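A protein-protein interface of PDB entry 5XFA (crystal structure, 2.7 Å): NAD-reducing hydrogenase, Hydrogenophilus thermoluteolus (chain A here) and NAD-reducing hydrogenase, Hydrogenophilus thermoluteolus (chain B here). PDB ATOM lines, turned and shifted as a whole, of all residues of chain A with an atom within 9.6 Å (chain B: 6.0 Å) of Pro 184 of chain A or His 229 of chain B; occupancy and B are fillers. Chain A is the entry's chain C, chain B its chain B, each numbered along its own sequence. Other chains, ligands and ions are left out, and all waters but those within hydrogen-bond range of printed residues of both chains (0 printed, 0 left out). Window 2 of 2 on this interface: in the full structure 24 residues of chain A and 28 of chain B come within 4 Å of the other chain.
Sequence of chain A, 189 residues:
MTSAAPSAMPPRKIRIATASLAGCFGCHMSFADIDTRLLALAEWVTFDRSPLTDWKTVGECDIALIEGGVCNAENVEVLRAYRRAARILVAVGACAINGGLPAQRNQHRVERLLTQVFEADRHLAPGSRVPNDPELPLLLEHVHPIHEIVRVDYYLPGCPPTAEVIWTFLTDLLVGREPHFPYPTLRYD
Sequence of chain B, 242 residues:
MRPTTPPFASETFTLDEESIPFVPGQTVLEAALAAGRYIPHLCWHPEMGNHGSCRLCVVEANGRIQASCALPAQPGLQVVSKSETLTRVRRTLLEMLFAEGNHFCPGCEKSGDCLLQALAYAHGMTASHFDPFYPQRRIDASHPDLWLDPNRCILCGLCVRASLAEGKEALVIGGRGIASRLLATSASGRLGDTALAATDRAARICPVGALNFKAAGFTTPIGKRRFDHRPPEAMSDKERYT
Tyr 183 of chain A touches Arg 230 of chain B. Pro 184 of chain A touches His 229 of chain B.
Hydrophobic or aromatic side chains of chain A within 4 Å of the printed part of chain B: Tyr 183. Of the 7 printed residues of chain B, 4 touch a printed residue of chain A. Printed residues of chain B that touch a printed residue of chain A: Arg 225, His 229, Arg 230 and Pro 231. Hydrophobic or aromatic side chains of chain B that line the printed part of chain A: His 229 and Pro 231. Among the printed residues, 4 pairs touch across the chains. Among the printed residues, Asp or Glu carboxylates within 4 Å of a Lys or Arg side-chain nitrogen of the other chain: Asp 189 of chain A with Arg 225 of chain B (3.1 Å).
The side-chain carboxylate (OD2) of Asp 189 of chain A lies within salt-bridge range of the guanidinium group (NH1) of Arg 225 of chain B (3.1 Å). The side-chain hydroxyl (OH) of Tyr 183 of chain A sits close to the backbone nitrogen (N) of Pro 231 of chain B (3.5 Å).
Of chain B, only His 229 comes within 4 Å of Pro 184 of chain A. Of the printed residues of chain A, His 229 of chain B touches Pro 184. Printed residues of chain A within 4 Å of Arg 230 of chain B: Tyr 183 (3.7 Å). Of the printed residues of chain B, Tyr 183 of chain A touches Arg 230 and Pro 231. Glu 164 of chain A touches none of the printed residues of chain B. The nearest printed residue of chain B that does not touch Pro 184 of chain A is Asp 228 of chain B (8.1 Å). The nearest printed residue of chain A that does not touch Arg 230 of chain B is Pro 184 of chain A (8.2 Å).
O of Arg 225 of chain B lies within hydrogen-bond range of NH1 of Arg 230 of chain B (3.2 Å). NE of Arg 187 of chain A is in salt-bridge range of OXT of Asp 189 of chain A (3.5 Å). OD2 of Asp 228 of chain B is in salt-bridge range of NE of Arg 225 of chain B (2.8 Å).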
ATOM      1  N   THR A 162      32.666  13.753   0.937  1.00  0.00           N
ATOM      2  CA  THR A 162      32.066  15.086   0.903  1.00  0.00           C
ATOM      3  C   THR A 162      33.126  16.178   0.694  1.00  0.00           C
ATOM      4  O   THR A 162      34.275  16.021   1.067  1.00  0.00           O
ATOM      5  CB  THR A 162      31.315  15.383   2.200  1.00  0.00           C
ATOM      6  OG1 THR A 162      32.154  15.065   3.317  1.00  0.00           O
ATOM      7  CG2 THR A 162      30.062  14.543   2.278  1.00  0.00           C
ATOM      8  N   ALA A 163      32.756  17.282   0.068  1.00  0.00           N
ATOM      9  CA  ALA A 163      33.690  18.393  -0.043  1.00  0.00           C
ATOM     10  C   ALA A 163      34.086  18.824   1.355  1.00  0.00           C
ATOM     11  O   ALA A 163      35.219  19.253   1.567  1.00  0.00           O
ATOM     12  CB  ALA A 163      33.084  19.562  -0.805  1.00  0.00           C
ATOM     13  N   GLU A 164      33.165  18.699   2.309  1.00  0.00           N
ATOM     14  CA  GLU A 164      33.450  19.120   3.682  1.00  0.00           C
ATOM     15  C   GLU A 164      34.506  18.280   4.367  1.00  0.00           C
ATOM     16  O   GLU A 164      35.222  18.764   5.236  1.00  0.00           O
ATOM     17  CB  GLU A 164      32.181  19.119   4.527  1.00  0.00           C
ATOM     18  CG  GLU A 164      32.303  19.914   5.807  1.00  0.00           C
ATOM     19  CD  GLU A 164      32.695  21.364   5.562  1.00  0.00           C
ATOM     20  OE1 GLU A 164      32.471  21.869   4.421  1.00  0.00           O
ATOM     21  OE2 GLU A 164      33.230  21.983   6.514  1.00  0.00           O
ATOM     22  N   VAL A 165      34.594  17.021   3.996  1.00  0.00           N
ATOM     23  CA  VAL A 165      35.670  16.170   4.479  1.00  0.00           C
ATOM     24  C   VAL A 165      36.960  16.560   3.789  1.00  0.00           C
ATOM     25  O   VAL A 165      37.973  16.809   4.431  1.00  0.00           O
ATOM     26  CB  VAL A 165      35.367  14.679   4.232  1.00  0.00           C
ATOM     27  CG1 VAL A 165      36.633  13.839   4.274  1.00  0.00           C
ATOM     28  CG2 VAL A 165      34.399  14.194   5.274  1.00  0.00           C
ATOM     29  N   THR A 168      38.153  19.663   5.361  1.00  0.00           N
ATOM     30  CA  THR A 168      38.595  19.502   6.720  1.00  0.00           C
ATOM     31  C   THR A 168      39.952  18.819   6.725  1.00  0.00           C
ATOM     32  O   THR A 168      40.843  19.223   7.452  1.00  0.00           O
ATOM     33  CB  THR A 168      37.560  18.718   7.523  1.00  0.00           C
ATOM     34  OG1 THR A 168      36.538  19.626   7.943  1.00  0.00           O
ATOM     35  CG2 THR A 168      38.182  18.048   8.739  1.00  0.00           C
ATOM     36  N   HIS A 180      40.995  14.782  11.732  1.00  0.00           N
ATOM     37  CA  HIS A 180      39.852  14.336  12.514  1.00  0.00           C
ATOM     38  C   HIS A 180      38.624  14.461  11.632  1.00  0.00           C
ATOM     39  O   HIS A 180      38.387  15.532  11.064  1.00  0.00           O
ATOM     40  CB  HIS A 180      39.682  15.203  13.769  1.00  0.00           C
ATOM     41  CG  HIS A 180      38.342  15.060  14.435  1.00  0.00           C
ATOM     42  ND1 HIS A 180      37.855  13.848  14.881  1.00  0.00           N
ATOM     43  CD2 HIS A 180      37.393  15.980  14.739  1.00  0.00           C
ATOM     44  CE1 HIS A 180      36.664  14.027  15.427  1.00  0.00           C
ATOM     45  NE2 HIS A 180      36.361  15.311  15.352  1.00  0.00           N
ATOM     46  N   PHE A 181      37.861  13.370  11.521  1.00  0.00           N
ATOM     47  CA  PHE A 181      36.611  13.360  10.763  1.00  0.00           C
ATOM     48  C   PHE A 181      35.417  13.169  11.691  1.00  0.00           C
ATOM     49  O   PHE A 181      35.222  12.082  12.243  1.00  0.00           O
ATOM     50  CB  PHE A 181      36.629  12.254   9.703  1.00  0.00           C
ATOM     51  CG  PHE A 181      37.791  12.344   8.749  1.00  0.00           C
ATOM     52  CD1 PHE A 181      38.059  13.532   8.064  1.00  0.00           C
ATOM     53  CD2 PHE A 181      38.616  11.238   8.530  1.00  0.00           C
ATOM     54  CE1 PHE A 181      39.130  13.617   7.192  1.00  0.00           C
ATOM     55  CE2 PHE A 181      39.685  11.314   7.654  1.00  0.00           C
ATOM     56  CZ  PHE A 181      39.942  12.507   6.985  1.00  0.00           C
ATOM     57  N   PRO A 182      34.613  14.231  11.874  1.00  0.00           N
ATOM     58  CA  PRO A 182      33.379  14.070  12.658  1.00  0.00           C
ATOM     59  C   PRO A 182      32.371  13.080  12.011  1.00  0.00           C
ATOM     60  O   PRO A 182      32.215  13.083  10.784  1.00  0.00           O
ATOM     61  CB  PRO A 182      32.801  15.504  12.713  1.00  0.00           C
ATOM     62  CG  PRO A 182      33.920  16.421  12.323  1.00  0.00           C
ATOM     63  CD  PRO A 182      34.804  15.624  11.415  1.00  0.00           C
ATOM     64  N   TYR A 183      31.702  12.252  12.826  1.00  0.00           N
ATOM     65  CA  TYR A 183      30.622  11.374  12.343  1.00  0.00           C
ATOM     66  C   TYR A 183      29.790  12.013  11.200  1.00  0.00           C
ATOM     67  O   TYR A 183      29.714  11.455  10.112  1.00  0.00           O
ATOM     68  CB  TYR A 183      29.723  10.953  13.507  1.00  0.00           C
ATOM     69  CG  TYR A 183      28.664   9.911  13.185  1.00  0.00           C
ATOM     70  CD1 TYR A 183      28.903   8.555  13.431  1.00  0.00           C
ATOM     71  CD2 TYR A 183      27.407  10.276  12.679  1.00  0.00           C
ATOM     72  CE1 TYR A 183      27.939   7.588  13.164  1.00  0.00           C
ATOM     73  CE2 TYR A 183      26.433   9.310  12.406  1.00  0.00           C
ATOM     74  CZ  TYR A 183      26.704   7.965  12.649  1.00  0.00           C
ATOM     75  OH  TYR A 183      25.765   6.978  12.386  1.00  0.00           O
ATOM     76  N   PRO A 184      29.226  13.220  11.411  1.00  0.00           N
ATOM     77  CA  PRO A 184      28.409  13.861  10.357  1.00  0.00           C
ATOM     78  C   PRO A 184      29.072  14.175   8.996  1.00  0.00           C
ATOM     79  O   PRO A 184      28.390  14.670   8.095  1.00  0.00           O
ATOM     80  CB  PRO A 184      27.990  15.195  11.000  1.00  0.00           C
ATOM     81  CG  PRO A 184      28.100  14.965  12.462  1.00  0.00           C
ATOM     82  CD  PRO A 184      29.295  14.075  12.612  1.00  0.00           C
ATOM     83  N   THR A 185      30.373  13.933   8.851  1.00  0.00           N
ATOM     84  CA  THR A 185      31.043  14.119   7.560  1.00  0.00           C
ATOM     85  C   THR A 185      31.402  12.763   6.917  1.00  0.00           C
ATOM     86  O   THR A 185      31.822  12.702   5.758  1.00  0.00           O
ATOM     87  CB  THR A 185      32.288  15.027   7.707  1.00  0.00           C
ATOM     88  OG1 THR A 185      33.312  14.360   8.463  1.00  0.00           O
ATOM     89  CG2 THR A 185      31.914  16.350   8.378  1.00  0.00           C
ATOM     90  N   LEU A 186      31.170  11.680   7.656  1.00  0.00           N
ATOM     91  CA  LEU A 186      31.595  10.358   7.249  1.00  0.00           C
ATOM     92  C   LEU A 186      30.547   9.646   6.389  1.00  0.00           C
ATOM     93  O   LEU A 186      29.366   9.545   6.755  1.00  0.00           O
ATOM     94  CB  LEU A 186      31.911   9.522   8.490  1.00  0.00           C
ATOM     95  CG  LEU A 186      33.205   8.722   8.427  1.00  0.00           C
ATOM     96  CD1 LEU A 186      34.407   9.635   8.226  1.00  0.00           C
ATOM     97  CD2 LEU A 186      33.360   7.910   9.702  1.00  0.00           C
ATOM     98  N   ARG A 187      30.986   9.169   5.230  1.00  0.00           N
ATOM     99  CA  ARG A 187      30.167   8.288   4.414  1.00  0.00           C
ATOM    100  C   ARG A 187      31.028   7.381   3.526  1.00  0.00           C
ATOM    101  O   ARG A 187      32.189   7.648   3.242  1.00  0.00           O
ATOM    102  CB  ARG A 187      29.173   9.082   3.580  1.00  0.00           C
ATOM    103  CG  ARG A 187      29.809   9.990   2.521  1.00  0.00           C
ATOM    104  CD  ARG A 187      28.853  10.272   1.351  1.00  0.00           C
ATOM    105  NE  ARG A 187      29.446  11.166   0.357  1.00  0.00           N
ATOM    106  CZ  ARG A 187      28.922  12.318  -0.079  1.00  0.00           C
ATOM    107  NH1 ARG A 187      27.742  12.749   0.349  1.00  0.00           N
ATOM    108  NH2 ARG A 187      29.582  13.045  -0.981  1.00  0.00           N
ATOM    109  N   ASP A 189      29.324   6.109   0.776  1.00  0.00           N
ATOM    110  CA  ASP A 189      28.429   5.974  -0.364  1.00  0.00           C
ATOM    111  C   ASP A 189      28.269   7.288  -1.173  1.00  0.00           C
ATOM    112  O   ASP A 189      27.163   7.594  -1.669  1.00  0.00           O
ATOM    113  CB  ASP A 189      27.085   5.443   0.119  1.00  0.00           C
ATOM    114  CG  ASP A 189      26.409   6.352   1.121  1.00  0.00           C
ATOM    115  OD1 ASP A 189      27.025   7.344   1.614  1.00  0.00           O
ATOM    116  OD2 ASP A 189      25.228   6.055   1.419  1.00  0.00           O
ATOM    117  OXT ASP A 189      29.251   8.065  -1.356  1.00  0.00           O
ATOM    118  N   GLY B 223      19.545  11.288   3.169  1.00  0.00           N
ATOM    119  CA  GLY B 223      19.188  12.223   4.237  1.00  0.00           C
ATOM    120  C   GLY B 223      18.123  11.690   5.178  1.00  0.00           C
ATOM    121  O   GLY B 223      18.016  12.159   6.316  1.00  0.00           O
ATOM    122  N   ARG B 225      17.286   8.159   5.479  1.00  0.00           N
ATOM    123  CA  ARG B 225      17.405   6.738   5.643  1.00  0.00           C
ATOM    124  C   ARG B 225      17.533   6.410   7.118  1.00  0.00           C
ATOM    125  O   ARG B 225      18.005   7.216   7.908  1.00  0.00           O
ATOM    126  CB  ARG B 225      18.571   6.194   4.792  1.00  0.00           C
ATOM    127  CG  ARG B 225      18.261   6.304   3.294  1.00  0.00           C
ATOM    128  CD  ARG B 225      19.476   6.362   2.365  1.00  0.00           C
ATOM    129  NE  ARG B 225      20.605   7.152   2.873  1.00  0.00           N
ATOM    130  CZ  ARG B 225      21.840   7.088   2.384  1.00  0.00           C
ATOM    131  NH1 ARG B 225      22.137   6.309   1.352  1.00  0.00           N
ATOM    132  NH2 ARG B 225      22.793   7.786   2.952  1.00  0.00           N
ATOM    133  N   PHE B 227      19.491   5.058   9.248  1.00  0.00           N
ATOM    134  CA  PHE B 227      20.686   5.482  10.016  1.00  0.00           C
ATOM    135  C   PHE B 227      21.346   6.819   9.622  1.00  0.00           C
ATOM    136  O   PHE B 227      22.415   7.102  10.142  1.00  0.00           O
ATOM    137  CB  PHE B 227      21.779   4.433   9.891  1.00  0.00           C
ATOM    138  CG  PHE B 227      21.418   3.142  10.505  1.00  0.00           C
ATOM    139  CD1 PHE B 227      21.547   2.951  11.873  1.00  0.00           C
ATOM    140  CD2 PHE B 227      20.903   2.116   9.736  1.00  0.00           C
ATOM    141  CE1 PHE B 227      21.180   1.760  12.459  1.00  0.00           C
ATOM    142  CE2 PHE B 227      20.547   0.919  10.319  1.00  0.00           C
ATOM    143  CZ  PHE B 227      20.682   0.744  11.684  1.00  0.00           C
ATOM    144  N   ASP B 228      20.738   7.617   8.734  1.00  0.00           N
ATOM    145  CA  ASP B 228      21.336   8.866   8.257  1.00  0.00           C
ATOM    146  C   ASP B 228      21.456   9.891   9.391  1.00  0.00           C
ATOM    147  O   ASP B 228      20.480  10.558   9.785  1.00  0.00           O
ATOM    148  CB  ASP B 228      20.506   9.471   7.116  1.00  0.00           C
ATOM    149  CG  ASP B 228      20.888   8.911   5.747  1.00  0.00           C
ATOM    150  OD1 ASP B 228      21.961   8.242   5.660  1.00  0.00           O
ATOM    151  OD2 ASP B 228      20.118   9.140   4.755  1.00  0.00           O
ATOM    152  N   HIS B 229      22.680  10.021   9.896  1.00  0.00           N
ATOM    153  CA  HIS B 229      22.990  10.890  11.031  1.00  0.00           C
ATOM    154  C   HIS B 229      22.341  10.458  12.357  1.00  0.00           C
ATOM    155  O   HIS B 229      22.115  11.291  13.252  1.00  0.00           O
ATOM    156  CB  HIS B 229      22.668  12.347  10.693  1.00  0.00           C
ATOM    157  CG  HIS B 229      23.425  12.864   9.515  1.00  0.00           C
ATOM    158  ND1 HIS B 229      22.816  13.196   8.323  1.00  0.00           N
ATOM    159  CD2 HIS B 229      24.749  13.079   9.338  1.00  0.00           C
ATOM    160  CE1 HIS B 229      23.733  13.606   7.467  1.00  0.00           C
ATOM    161  NE2 HIS B 229      24.915  13.546   8.058  1.00  0.00           N
ATOM    162  N   ARG B 230      22.086   9.147  12.478  1.00  0.00           N
ATOM    163  CA  ARG B 230      21.589   8.533  13.708  1.00  0.00           C
ATOM    164  C   ARG B 230      22.389   7.295  13.965  1.00  0.00           C
ATOM    165  O   ARG B 230      22.119   6.273  13.334  1.00  0.00           O
ATOM    166  CB  ARG B 230      20.148   8.062  13.544  1.00  0.00           C
ATOM    167  CG  ARG B 230      19.129   9.109  13.156  1.00  0.00           C
ATOM    168  CD  ARG B 230      17.756   8.468  13.136  1.00  0.00           C
ATOM    169  NE  ARG B 230      16.692   9.362  12.687  1.00  0.00           N
ATOM    170  CZ  ARG B 230      16.237   9.450  11.445  1.00  0.00           C
ATOM    171  NH1 ARG B 230      16.777   8.742  10.460  1.00  0.00           N
ATOM    172  NH2 ARG B 230      15.225  10.267  11.192  1.00  0.00           N
ATOM    173  N   PRO B 231      23.379   7.350  14.874  1.00  0.00           N
ATOM    174  CA  PRO B 231      24.047   6.077  15.184  1.00  0.00           C
ATOM    175  C   PRO B 231      23.086   5.122  15.895  1.00  0.00           C
ATOM    176  O   PRO B 231      22.012   5.537  16.325  1.00  0.00           O
ATOM    177  CB  PRO B 231      25.221   6.489  16.082  1.00  0.00           C
ATOM    178  CG  PRO B 231      24.849   7.827  16.617  1.00  0.00           C
ATOM    179  CD  PRO B 231      24.004   8.488  15.568  1.00  0.00           C
